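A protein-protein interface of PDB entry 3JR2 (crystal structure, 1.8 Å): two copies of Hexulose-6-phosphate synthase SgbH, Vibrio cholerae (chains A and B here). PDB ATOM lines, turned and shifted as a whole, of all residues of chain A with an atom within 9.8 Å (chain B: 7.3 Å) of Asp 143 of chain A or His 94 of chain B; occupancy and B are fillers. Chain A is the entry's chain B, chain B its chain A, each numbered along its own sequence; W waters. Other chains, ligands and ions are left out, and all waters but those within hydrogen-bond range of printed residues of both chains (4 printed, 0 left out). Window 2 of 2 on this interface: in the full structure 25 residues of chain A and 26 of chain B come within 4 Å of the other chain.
Among the printed residues, pairs that only touch across the chains: Lys 67 of chain A with Thr 69 of chain B (3.9 Å), Ala 92 of chain A with Ala 92 of chain B (3.4 Å), Tyr 117 of chain A with Thr 69 of chain B (3.4 Å), Tyr 117 of chain A with Ala 92 of chain B (3.7 Å), Arg 142 of chain A with His 94 of chain B (3.5 Å) and Arg 142 of chain A with Ala 96 of chain B (3.5 Å).
Of the 24 printed residues of chain A, 6 touch a printed residue of chain B. Of the 16 printed residues of chain B, 6 touch a printed residue of chain A. Hydrophobic or aromatic side chains of chain B within 4 Å of the printed part of chain A: Ala 92, His 94 and Ala 96. Among the printed residues, 10 pairs touch across the chains. Among the printed residues, no Asp or Glu carboxylate lies within 4 Å of a Lys or Arg side-chain nitrogen of the other chain.
The backbone carbonyl oxygen (O) of Ala 92 of chain B is in hydrogen-bond range of the backbone NH (N) of Gly 118 of chain A, 3.4 Å away. The side-chain hydroxyl (OG1) of Thr 97 of chain B is in hydrogen-bond range of the guanidinium group (NH2) of Arg 142 of chain A (3.1 Å). A ring nitrogen (NE2) of His 94 of chain B sits at hydrogen-bond distance from the side-chain carboxylate of Asp 143 of chain A (3.1 Å). OD2 of Asp 70 of chain B sits at hydrogen-bond distance from OH of Tyr 117 of chain A (2.6 Å).
Of chain B, only His 94 (3.1 Å) comes within 4 Å of Asp 143 of chain A. His 94 of chain B touches just these residues of chain A: Arg 142 (3.5 Å) and Asp 143 (3.1 Å). Ala 93 of chain B touches none of the printed residues of chain A. Ala 96 of chain B touches just one residue of chain A: Arg 142. Thr 97 of chain B touches one residue of chain A. Of the printed residues of chain B, Arg 142 of chain A touches His 94, Ala 96 and Thr 97. Of the printed residues of chain A, Thr 69 of chain B touches Lys 67 and Tyr 117. The nearest residue of chain B that does not touch Asp 143 of chain A is Ile 95 of chain B (5.8 Å). The nearest residue of chain A that does not touch His 94 of chain B is Leu 146 of chain A (4.3 Å). The nearest printed residue of chain B that does not touch Arg 142 of chain A is Asp 70 of chain B (4.4 Å).
Ala 92 of chain B touches its own counterpart, Ala 92 of chain A. Positions printed for both chains: 90 and 92. Of the 10 pairs that touch across the chains among the printed residues, 1 has its exchanged pair printed and touching as well.
Water W3 bridges O of Lys 67 of chain A (2.7 Å) and OG1 of Thr 69 of chain B (3.2 Å). Water W1 lies within hydrogen-bond range of O of Ala 92 of chain B (2.7 Å), N of Gly 118 of chain A (2.9 Å) and N of His 94 of chain B (3.3 Å). Water W4 lies within hydrogen-bond range of the side-chain carboxylate of Asp 70 of chain B (2.8 Å) and the side-chain hydroxyl of Tyr 117 of chain A (3.3 Å). Water W2 lies within hydrogen-bond range of OG of Ser 90 of chain A, OG1 of Thr 69 of chain B and OG of Ser 90 of chain B.
The backbone NH (N) of Ala 92 of chain A sits close to the side-chain hydroxyl (OG) of Ser 90 of chain A, 3.1 Å away. The backbone NH (N) of Ala 96 of chain B sits at hydrogen-bond distance from a ring nitrogen (ND1) of His 94 of chain B (2.9 Å). OH of Tyr 117 of chain A lies close to NE2 of His 139 of chain A (3.3 Å). OG of Ser 141 of chain A sits at hydrogen-bond distance from N of Asp 143 of chain A (3.1 Å). N of Ala 92 of chain B sits close to OG of Ser 90 of chain B, 3.0 Å away.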
ATOM      1  N   LYS A  67      10.485   5.447   2.589  1.00  0.00           N
ATOM      2  CA  LYS A  67      11.656   5.777   1.743  1.00  0.00           C
ATOM      3  C   LYS A  67      11.205   6.000   0.270  1.00  0.00           C
ATOM      4  O   LYS A  67      11.784   5.467  -0.676  1.00  0.00           O
ATOM      5  CB  LYS A  67      12.738   4.711   1.829  1.00  0.00           C
ATOM      6  CG  LYS A  67      13.269   4.606   3.270  1.00  0.00           C
ATOM      7  CD  LYS A  67      14.431   3.634   3.367  1.00  0.00           C
ATOM      8  CE  LYS A  67      14.835   3.280   4.757  1.00  0.00           C
ATOM      9  NZ  LYS A  67      13.736   2.969   5.658  1.00  0.00           N
ATOM     10  N   SER A  90      12.889   9.085   0.008  1.00  0.00           N
ATOM     11  CA  SER A  90      14.288   8.871  -0.308  1.00  0.00           C
ATOM     12  C   SER A  90      14.923  10.136  -0.918  1.00  0.00           C
ATOM     13  O   SER A  90      14.317  10.805  -1.738  1.00  0.00           O
ATOM     14  CB  SER A  90      14.386   7.721  -1.327  1.00  0.00           C
ATOM     15  OG  SER A  90      15.750   7.495  -1.624  1.00  0.00           O
ATOM     16  N   ALA A  92      16.909   9.909  -3.129  1.00  0.00           N
ATOM     17  CA  ALA A  92      17.017   9.501  -4.534  1.00  0.00           C
ATOM     18  C   ALA A  92      15.751   9.787  -5.348  1.00  0.00           C
ATOM     19  O   ALA A  92      15.768   9.662  -6.575  1.00  0.00           O
ATOM     20  CB  ALA A  92      17.409   8.030  -4.645  1.00  0.00           C
ATOM     21  N   ILE A 116      18.320   9.998   4.002  1.00  0.00           N
ATOM     22  CA  ILE A 116      19.604  10.267   3.298  1.00  0.00           C
ATOM     23  C   ILE A 116      20.319   8.964   2.916  1.00  0.00           C
ATOM     24  O   ILE A 116      20.899   8.280   3.748  1.00  0.00           O
ATOM     25  CB  ILE A 116      20.497  11.197   4.074  1.00  0.00           C
ATOM     26  CG1 ILE A 116      19.795  12.531   4.358  1.00  0.00           C
ATOM     27  CG2 ILE A 116      21.826  11.433   3.333  1.00  0.00           C
ATOM     28  CD1 ILE A 116      20.636  13.442   5.265  1.00  0.00           C
ATOM     29  N   TYR A 117      20.214   8.656   1.616  1.00  0.00           N
ATOM     30  CA  TYR A 117      20.811   7.503   0.943  1.00  0.00           C
ATOM     31  C   TYR A 117      21.335   7.927  -0.419  1.00  0.00           C
ATOM     32  O   TYR A 117      20.872   8.898  -1.016  1.00  0.00           O
ATOM     33  CB  TYR A 117      19.802   6.345   0.703  1.00  0.00           C
ATOM     34  CG  TYR A 117      19.392   5.578   1.968  1.00  0.00           C
ATOM     35  CD1 TYR A 117      20.096   4.456   2.376  1.00  0.00           C
ATOM     36  CD2 TYR A 117      18.347   6.015   2.762  1.00  0.00           C
ATOM     37  CE1 TYR A 117      19.781   3.803   3.554  1.00  0.00           C
ATOM     38  CE2 TYR A 117      18.021   5.374   3.926  1.00  0.00           C
ATOM     39  CZ  TYR A 117      18.729   4.258   4.308  1.00  0.00           C
ATOM     40  OH  TYR A 117      18.431   3.587   5.491  1.00  0.00           O
ATOM     41  N   GLY A 118      22.300   7.187  -0.910  1.00  0.00           N
ATOM     42  CA  GLY A 118      22.747   7.291  -2.314  1.00  0.00           C
ATOM     43  C   GLY A 118      23.866   8.303  -2.448  1.00  0.00           C
ATOM     44  O   GLY A 118      24.503   8.695  -1.477  1.00  0.00           O
ATOM     45  N   ASN A 119      24.061   8.774  -3.663  1.00  0.00           N
ATOM     46  CA  ASN A 119      25.117   9.755  -3.995  1.00  0.00           C
ATOM     47  C   ASN A 119      24.526  11.114  -3.871  1.00  0.00           C
ATOM     48  O   ASN A 119      24.518  11.929  -4.808  1.00  0.00           O
ATOM     49  CB  ASN A 119      25.600   9.512  -5.447  1.00  0.00           C
ATOM     50  CG  ASN A 119      26.122   8.066  -5.703  1.00  0.00           C
ATOM     51  OD1 ASN A 119      25.932   7.516  -6.783  1.00  0.00           O
ATOM     52  ND2 ASN A 119      26.779   7.479  -4.724  1.00  0.00           N
ATOM     53  N   HIS A 139      21.870   8.415   8.679  1.00  0.00           N
ATOM     54  CA  HIS A 139      22.320   7.123   9.144  1.00  0.00           C
ATOM     55  C   HIS A 139      23.823   7.108   9.223  1.00  0.00           C
ATOM     56  O   HIS A 139      24.481   7.508   8.271  1.00  0.00           O
ATOM     57  CB  HIS A 139      21.918   6.020   8.149  1.00  0.00           C
ATOM     58  CG  HIS A 139      20.441   5.928   7.950  1.00  0.00           C
ATOM     59  ND1 HIS A 139      19.663   4.980   8.571  1.00  0.00           N
ATOM     60  CD2 HIS A 139      19.592   6.716   7.237  1.00  0.00           C
ATOM     61  CE1 HIS A 139      18.395   5.173   8.226  1.00  0.00           C
ATOM     62  NE2 HIS A 139      18.331   6.217   7.415  1.00  0.00           N
ATOM     63  N   ARG A 140      24.343   6.511  10.280  1.00  0.00           N
ATOM     64  CA  ARG A 140      25.767   6.266  10.371  1.00  0.00           C
ATOM     65  C   ARG A 140      26.188   5.539   9.098  1.00  0.00           C
ATOM     66  O   ARG A 140      25.490   4.571   8.653  1.00  0.00           O
ATOM     67  CB  ARG A 140      26.123   5.433  11.611  1.00  0.00           C
ATOM     68  CG  ARG A 140      27.640   5.308  11.811  1.00  0.00           C
ATOM     69  CD  ARG A 140      28.012   4.850  13.211  1.00  0.00           C
ATOM     70  NE  ARG A 140      27.538   3.508  13.491  1.00  0.00           N
ATOM     71  CZ  ARG A 140      27.456   2.962  14.700  1.00  0.00           C
ATOM     72  NH1 ARG A 140      26.979   1.726  14.817  1.00  0.00           N
ATOM     73  NH2 ARG A 140      27.816   3.644  15.782  1.00  0.00           N
ATOM     74  N   SER A 141      27.296   6.013   8.515  1.00  0.00           N
ATOM     75  CA  SER A 141      27.880   5.392   7.326  1.00  0.00           C
ATOM     76  C   SER A 141      27.910   3.869   7.409  1.00  0.00           C
ATOM     77  O   SER A 141      28.440   3.271   8.363  1.00  0.00           O
ATOM     78  CB  SER A 141      29.338   5.879   7.120  1.00  0.00           C
ATOM     79  OG  SER A 141      29.982   5.070   6.171  1.00  0.00           O
ATOM     80  N   ARG A 142      27.348   3.212   6.390  1.00  0.00           N
ATOM     81  CA  ARG A 142      27.404   1.753   6.285  1.00  0.00           C
ATOM     82  C   ARG A 142      28.865   1.253   6.231  1.00  0.00           C
ATOM     83  O   ARG A 142      29.218   0.231   6.842  1.00  0.00           O
ATOM     84  CB  ARG A 142      26.625   1.279   5.054  1.00  0.00           C
ATOM     85  CG  ARG A 142      26.622  -0.265   4.907  1.00  0.00           C
ATOM     86  CD  ARG A 142      25.961  -0.949   6.095  1.00  0.00           C
ATOM     87  NE  ARG A 142      25.803  -2.399   5.869  1.00  0.00           N
ATOM     88  CZ  ARG A 142      24.856  -2.948   5.097  1.00  0.00           C
ATOM     89  NH1 ARG A 142      24.830  -4.247   4.928  1.00  0.00           N
ATOM     90  NH2 ARG A 142      24.002  -2.212   4.427  1.00  0.00           N
ATOM     91  N   ASP A 143      29.738   2.021   5.610  1.00  0.00           N
ATOM     92  CA  ASP A 143      31.170   1.632   5.604  1.00  0.00           C
ATOM     93  C   ASP A 143      31.772   1.663   6.980  1.00  0.00           C
ATOM     94  O   ASP A 143      32.598   0.792   7.298  1.00  0.00           O
ATOM     95  CB  ASP A 143      31.927   2.467   4.613  1.00  0.00           C
ATOM     96  CG  ASP A 143      31.338   2.329   3.242  1.00  0.00           C
ATOM     97  OD1 ASP A 143      31.418   1.206   2.697  1.00  0.00           O
ATOM     98  OD2 ASP A 143      30.656   3.253   2.792  1.00  0.00           O
ATOM     99  N   ALA A 144      31.383   2.635   7.810  1.00  0.00           N
ATOM    100  CA  ALA A 144      31.834   2.669   9.208  1.00  0.00           C
ATOM    101  C   ALA A 144      31.361   1.429   9.975  1.00  0.00           C
ATOM    102  O   ALA A 144      32.139   0.781  10.718  1.00  0.00           O
ATOM    103  CB  ALA A 144      31.373   3.948   9.919  1.00  0.00           C
ATOM    104  N   GLU A 145      30.115   1.037   9.755  1.00  0.00           N
ATOM    105  CA  GLU A 145      29.582  -0.124  10.421  1.00  0.00           C
ATOM    106  C   GLU A 145      30.319  -1.362   9.963  1.00  0.00           C
ATOM    107  O   GLU A 145      30.668  -2.193  10.793  1.00  0.00           O
ATOM    108  CB  GLU A 145      28.083  -0.281  10.134  1.00  0.00           C
ATOM    109  CG  GLU A 145      27.265   0.811  10.707  1.00  0.00           C
ATOM    110  CD  GLU A 145      25.749   0.584  10.497  1.00  0.00           C
ATOM    111  OE1 GLU A 145      24.957   1.253  11.208  1.00  0.00           O
ATOM    112  OE2 GLU A 145      25.386  -0.246   9.625  1.00  0.00           O
ATOM    113  N   LEU A 146      30.582  -1.472   8.651  1.00  0.00           N
ATOM    114  CA  LEU A 146      31.239  -2.677   8.086  1.00  0.00           C
ATOM    115  C   LEU A 146      32.606  -2.826   8.739  1.00  0.00           C
ATOM    116  O   LEU A 146      33.003  -3.929   9.095  1.00  0.00           O
ATOM    117  CB  LEU A 146      31.369  -2.625   6.555  1.00  0.00           C
ATOM    118  CG  LEU A 146      30.037  -2.788   5.790  1.00  0.00           C
ATOM    119  CD1 LEU A 146      30.246  -2.379   4.372  1.00  0.00           C
ATOM    120  CD2 LEU A 146      29.440  -4.239   5.873  1.00  0.00           C
ATOM    121  N   ALA A 147      33.303  -1.706   8.940  1.00  0.00           N
ATOM    122  CA  ALA A 147      34.635  -1.721   9.582  1.00  0.00           C
ATOM    123  C   ALA A 147      34.601  -1.842  11.107  1.00  0.00           C
ATOM    124  O   ALA A 147      35.645  -2.024  11.713  1.00  0.00           O
ATOM    125  CB  ALA A 147      35.393  -0.476   9.201  1.00  0.00           C
ATOM    126  N   GLY A 148      33.438  -1.701  11.724  1.00  0.00           N
ATOM    127  CA  GLY A 148      33.286  -1.716  13.154  1.00  0.00           C
ATOM    128  C   GLY A 148      33.947  -0.553  13.865  1.00  0.00           C
ATOM    129  O   GLY A 148      34.475  -0.750  14.932  1.00  0.00           O
ATOM    130  N   ILE A 149      33.885   0.663  13.337  1.00  0.00           N
ATOM    131  CA  ILE A 149      34.708   1.750  13.923  1.00  0.00           C
ATOM    132  C   ILE A 149      34.000   2.900  14.660  1.00  0.00           C
ATOM    133  O   ILE A 149      34.653   3.836  15.188  1.00  0.00           O
ATOM    134  CB  ILE A 149      35.723   2.320  12.905  1.00  0.00           C
ATOM    135  CG1 ILE A 149      35.044   2.788  11.637  1.00  0.00           C
ATOM    136  CG2 ILE A 149      36.851   1.296  12.592  1.00  0.00           C
ATOM    137  CD1 ILE A 149      36.036   3.360  10.681  1.00  0.00           C
ATOM    138  N   GLY A 150      32.686   2.839  14.717  1.00  0.00           N
ATOM    139  CA  GLY A 150      31.901   3.847  15.442  1.00  0.00           C
ATOM    140  C   GLY A 150      31.676   5.037  14.528  1.00  0.00           C
ATOM    141  O   GLY A 150      31.719   4.871  13.330  1.00  0.00           O
ATOM    142  N   TRP A 151      31.416   6.229  15.080  1.00  0.00           N
ATOM    143  CA  TRP A 151      31.109   7.375  14.257  1.00  0.00           C
ATOM    144  C   TRP A 151      32.409   8.002  13.734  1.00  0.00           C
ATOM    145  O   TRP A 151      33.455   7.917  14.412  1.00  0.00           O
ATOM    146  CB  TRP A 151      30.299   8.425  15.037  1.00  0.00           C
ATOM    147  CG  TRP A 151      28.908   8.027  15.270  1.00  0.00           C
ATOM    148  CD1 TRP A 151      28.422   7.304  16.340  1.00  0.00           C
ATOM    149  CD2 TRP A 151      27.791   8.301  14.438  1.00  0.00           C
ATOM    150  NE1 TRP A 151      27.083   7.105  16.207  1.00  0.00           N
ATOM    151  CE2 TRP A 151      26.673   7.674  15.029  1.00  0.00           C
ATOM    152  CE3 TRP A 151      27.625   8.957  13.212  1.00  0.00           C
ATOM    153  CZ2 TRP A 151      25.401   7.766  14.481  1.00  0.00           C
ATOM    154  CZ3 TRP A 151      26.355   9.033  12.670  1.00  0.00           C
ATOM    155  CH2 TRP A 151      25.267   8.451  13.310  1.00  0.00           C
ATOM    156  N   THR A 152      32.361   8.580  12.538  1.00  0.00           N
ATOM    157  CA  THR A 152      33.510   9.281  11.998  1.00  0.00           C
ATOM    158  C   THR A 152      33.189  10.729  11.642  1.00  0.00           C
ATOM    159  O   THR A 152      32.018  11.111  11.529  1.00  0.00           O
ATOM    160  CB  THR A 152      34.076   8.545  10.771  1.00  0.00           C
ATOM    161  OG1 THR A 152      33.156   8.665   9.702  1.00  0.00           O
ATOM    162  CG2 THR A 152      34.319   7.021  11.068  1.00  0.00           C
ATOM    163  N   ASP A 154      33.538  12.412   8.927  1.00  0.00           N
ATOM    164  CA  ASP A 154      32.941  12.685   7.609  1.00  0.00           C
ATOM    165  C   ASP A 154      31.417  12.742   7.824  1.00  0.00           C
ATOM    166  O   ASP A 154      30.757  13.638   7.323  1.00  0.00           O
ATOM    167  CB  ASP A 154      33.286  11.567   6.621  1.00  0.00           C
ATOM    168  CG  ASP A 154      33.583  12.061   5.201  1.00  0.00           C
ATOM    169  OD1 ASP A 154      32.860  12.963   4.675  1.00  0.00           O
ATOM    170  OD2 ASP A 154      34.557  11.499   4.594  1.00  0.00           O
ATOM    171  N   ASP A 155      30.886  11.822   8.630  1.00  0.00           N
ATOM    172  CA  ASP A 155      29.431  11.877   8.999  1.00  0.00           C
ATOM    173  C   ASP A 155      29.145  13.138   9.834  1.00  0.00           C
ATOM    174  O   ASP A 155      28.212  13.873   9.558  1.00  0.00           O
ATOM    175  CB  ASP A 155      28.999  10.620   9.739  1.00  0.00           C
ATOM    176  CG  ASP A 155      28.676   9.461   8.788  1.00  0.00           C
ATOM    177  OD1 ASP A 155      28.498   9.722   7.579  1.00  0.00           O
ATOM    178  OD2 ASP A 155      28.548   8.325   9.284  1.00  0.00           O
ATOM    179  N   LYS A 158      29.162  16.284   7.687  1.00  0.00           N
ATOM    180  CA  LYS A 158      27.992  16.385   6.803  1.00  0.00           C
ATOM    181  C   LYS A 158      26.754  16.777   7.604  1.00  0.00           C
ATOM    182  O   LYS A 158      25.945  17.589   7.169  1.00  0.00           O
ATOM    183  CB  LYS A 158      27.783  15.086   5.977  1.00  0.00           C
ATOM    184  CG  LYS A 158      28.852  14.888   4.882  1.00  0.00           C
ATOM    185  CD  LYS A 158      28.880  13.453   4.363  1.00  0.00           C
ATOM    186  CE  LYS A 158      29.726  13.299   3.061  1.00  0.00           C
ATOM    187  NZ  LYS A 158      30.133  11.857   2.924  1.00  0.00           N
ATOM    188  N   THR B  68      13.838  -1.354  -2.796  1.00  0.00           N
ATOM    189  CA  THR B  68      14.598  -1.607  -1.554  1.00  0.00           C
ATOM    190  C   THR B  68      15.762  -0.650  -1.421  1.00  0.00           C
ATOM    191  O   THR B  68      16.642  -0.611  -2.273  1.00  0.00           O
ATOM    192  CB  THR B  68      15.140  -3.017  -1.559  1.00  0.00           C
ATOM    193  OG1 THR B  68      14.068  -3.891  -1.878  1.00  0.00           O
ATOM    194  CG2 THR B  68      15.669  -3.429  -0.128  1.00  0.00           C
ATOM    195  N   THR B  69      15.782   0.106  -0.337  1.00  0.00           N
ATOM    196  CA  THR B  69      16.851   1.033  -0.086  1.00  0.00           C
ATOM    197  C   THR B  69      17.726   0.656   1.100  1.00  0.00           C
ATOM    198  O   THR B  69      18.866   1.109   1.186  1.00  0.00           O
ATOM    199  CB  THR B  69      16.195   2.406   0.096  1.00  0.00           C
ATOM    200  OG1 THR B  69      15.545   2.741  -1.141  1.00  0.00           O
ATOM    201  CG2 THR B  69      17.199   3.516   0.377  1.00  0.00           C
ATOM    202  N   ASP B  70      17.193  -0.127   2.025  1.00  0.00           N
ATOM    203  CA  ASP B  70      17.950  -0.629   3.193  1.00  0.00           C
ATOM    204  C   ASP B  70      17.128  -1.828   3.732  1.00  0.00           C
ATOM    205  O   ASP B  70      16.042  -2.123   3.239  1.00  0.00           O
ATOM    206  CB  ASP B  70      18.075   0.499   4.268  1.00  0.00           C
ATOM    207  CG  ASP B  70      19.272   0.323   5.220  1.00  0.00           C
ATOM    208  OD1 ASP B  70      19.887  -0.764   5.193  1.00  0.00           O
ATOM    209  OD2 ASP B  70      19.638   1.328   5.923  1.00  0.00           O
ATOM    210  N   VAL B  89      15.367  -3.258  -6.282  1.00  0.00           N
ATOM    211  CA  VAL B  89      16.260  -2.664  -5.323  1.00  0.00           C
ATOM    212  C   VAL B  89      16.660  -1.299  -5.850  1.00  0.00           C
ATOM    213  O   VAL B  89      17.055  -1.175  -7.017  1.00  0.00           O
ATOM    214  CB  VAL B  89      17.479  -3.562  -5.152  1.00  0.00           C
ATOM    215  CG1 VAL B  89      18.486  -2.941  -4.220  1.00  0.00           C
ATOM    216  CG2 VAL B  89      17.070  -4.842  -4.569  1.00  0.00           C
ATOM    217  N   SER B  90      16.533  -0.260  -5.029  1.00  0.00           N
ATOM    218  CA  SER B  90      16.898   1.089  -5.479  1.00  0.00           C
ATOM    219  C   SER B  90      18.392   1.197  -5.770  1.00  0.00           C
ATOM    220  O   SER B  90      19.242   0.694  -5.018  1.00  0.00           O
ATOM    221  CB  SER B  90      16.551   2.149  -4.423  1.00  0.00           C
ATOM    222  OG  SER B  90      16.993   3.460  -4.834  1.00  0.00           O
ATOM    223  N   ALA B  91      18.729   1.916  -6.824  1.00  0.00           N
ATOM    224  CA  ALA B  91      20.069   2.254  -7.124  1.00  0.00           C
ATOM    225  C   ALA B  91      20.748   3.007  -5.976  1.00  0.00           C
ATOM    226  O   ALA B  91      21.966   3.070  -5.920  1.00  0.00           O
ATOM    227  CB  ALA B  91      20.134   3.122  -8.437  1.00  0.00           C
ATOM    228  N   ALA B  92      19.970   3.654  -5.127  1.00  0.00           N
ATOM    229  CA  ALA B  92      20.513   4.433  -3.991  1.00  0.00           C
ATOM    230  C   ALA B  92      20.799   3.578  -2.770  1.00  0.00           C
ATOM    231  O   ALA B  92      21.320   4.074  -1.757  1.00  0.00           O
ATOM    232  CB  ALA B  92      19.569   5.623  -3.625  1.00  0.00           C
ATOM    233  N   ALA B  93      20.419   2.294  -2.800  1.00  0.00           N
ATOM    234  CA  ALA B  93      20.811   1.405  -1.721  1.00  0.00           C
ATOM    235  C   ALA B  93      22.337   1.361  -1.635  1.00  0.00           C
ATOM    236  O   ALA B  93      23.020   1.338  -2.638  1.00  0.00           O
ATOM    237  CB  ALA B  93      20.236  -0.021  -1.926  1.00  0.00           C
ATOM    238  N   HIS B  94      22.883   1.313  -0.430  1.00  0.00           N
ATOM    239  CA  HIS B  94      24.289   1.042  -0.293  1.00  0.00           C
ATOM    240  C   HIS B  94      24.679  -0.292  -0.969  1.00  0.00           C
ATOM    241  O   HIS B  94      23.915  -1.260  -0.991  1.00  0.00           O
ATOM    242  CB  HIS B  94      24.686   1.025   1.165  1.00  0.00           C
ATOM    243  CG  HIS B  94      26.163   1.039   1.381  1.00  0.00           C
ATOM    244  ND1 HIS B  94      26.916  -0.111   1.373  1.00  0.00           N
ATOM    245  CD2 HIS B  94      27.015   2.056   1.659  1.00  0.00           C
ATOM    246  CE1 HIS B  94      28.188   0.210   1.582  1.00  0.00           C
ATOM    247  NE2 HIS B  94      28.270   1.522   1.750  1.00  0.00           N
ATOM    248  N   ILE B  95      25.862  -0.318  -1.567  1.00  0.00           N
ATOM    249  CA  ILE B  95      26.330  -1.546  -2.262  1.00  0.00           C
ATOM    250  C   ILE B  95      26.297  -2.813  -1.361  1.00  0.00           C
ATOM    251  O   ILE B  95      26.048  -3.911  -1.862  1.00  0.00           O
ATOM    252  CB  ILE B  95      27.684  -1.367  -2.982  1.00  0.00           C
ATOM    253  CG1 ILE B  95      27.942  -2.492  -3.971  1.00  0.00           C
ATOM    254  CG2 ILE B  95      28.851  -1.199  -1.940  1.00  0.00           C
ATOM    255  CD1 ILE B  95      27.038  -2.512  -5.234  1.00  0.00           C
ATOM    256  N   ALA B  96      26.482  -2.655  -0.036  1.00  0.00           N
ATOM    257  CA  ALA B  96      26.376  -3.789   0.874  1.00  0.00           C
ATOM    258  C   ALA B  96      24.957  -4.304   0.965  1.00  0.00           C
ATOM    259  O   ALA B  96      24.736  -5.505   1.198  1.00  0.00           O
ATOM    260  CB  ALA B  96      26.916  -3.468   2.282  1.00  0.00           C
ATOM    261  N   THR B  97      23.984  -3.405   0.869  1.00  0.00           N
ATOM    262  CA  THR B  97      22.559  -3.802   0.868  1.00  0.00           C
ATOM    263  C   THR B  97      22.249  -4.548  -0.385  1.00  0.00           C
ATOM    264  O   THR B  97      21.569  -5.590  -0.393  1.00  0.00           O
ATOM    265  CB  THR B  97      21.643  -2.544   1.021  1.00  0.00           C
ATOM    266  OG1 THR B  97      21.739  -2.062   2.377  1.00  0.00           O
ATOM    267  CG2 THR B  97      20.117  -2.900   0.671  1.00  0.00           C
ATOM    268  N   ILE B  98      22.716  -4.002  -1.490  1.00  0.00           N
ATOM    269  CA  ILE B  98      22.530  -4.624  -2.788  1.00  0.00           C
ATOM    270  C   ILE B  98      23.108  -6.037  -2.764  1.00  0.00           C
ATOM    271  O   ILE B  98      22.430  -6.980  -3.157  1.00  0.00           O
ATOM    272  CB  ILE B  98      23.075  -3.763  -3.935  1.00  0.00           C
ATOM    273  CG1 ILE B  98      22.383  -2.409  -3.906  1.00  0.00           C
ATOM    274  CG2 ILE B  98      22.866  -4.455  -5.299  1.00  0.00           C
ATOM    275  CD1 ILE B  98      22.823  -1.445  -5.014  1.00  0.00           C
ATOM    276  N   ALA B  99      24.310  -6.177  -2.226  1.00  0.00           N
ATOM    277  CA  ALA B  99      24.941  -7.503  -2.125  1.00  0.00           C
ATOM    278  C   ALA B  99      24.127  -8.467  -1.289  1.00  0.00           C
ATOM    279  O   ALA B  99      24.000  -9.668  -1.656  1.00  0.00           O
ATOM    280  CB  ALA B  99      26.384  -7.389  -1.585  1.00  0.00           C
ATOM    281  N   ALA B 100      23.565  -7.954  -0.181  1.00  0.00           N
ATOM    282  CA  ALA B 100      22.748  -8.748   0.745  1.00  0.00           C
ATOM    283  C   ALA B 100      21.515  -9.231   0.054  1.00  0.00           C
ATOM    284  O   ALA B 100      21.161 -10.391   0.219  1.00  0.00           O
ATOM    285  CB  ALA B 100      22.368  -7.923   1.997  1.00  0.00           C
ATOM    286  N   LEU B 131      28.402  -7.884  -8.918  1.00  0.00           N
ATOM    287  CA  LEU B 131      27.725  -8.721  -7.940  1.00  0.00           C
ATOM    288  C   LEU B 131      26.911  -9.770  -8.646  1.00  0.00           C
ATOM    289  O   LEU B 131      26.320 -10.597  -8.016  1.00  0.00           O
ATOM    290  CB  LEU B 131      26.771  -7.898  -7.071  1.00  0.00           C
ATOM    291  CG  LEU B 131      27.392  -6.942  -6.083  1.00  0.00           C
ATOM    292  CD1 LEU B 131      26.240  -6.119  -5.464  1.00  0.00           C
ATOM    293  CD2 LEU B 131      28.162  -7.803  -5.044  1.00  0.00           C
HETATM  294  O   HOH W   1      23.194   4.588   0.158  1.00  0.00           O
HETATM  295  O   HOH W   2      15.609   4.985  -2.864  1.00  0.00           O
HETATM  296  O   HOH W   3      12.404   2.964  -1.551  1.00  0.00           O
HETATM  297  O   HOH W   4      21.625   3.278   6.071  1.00  0.00           O
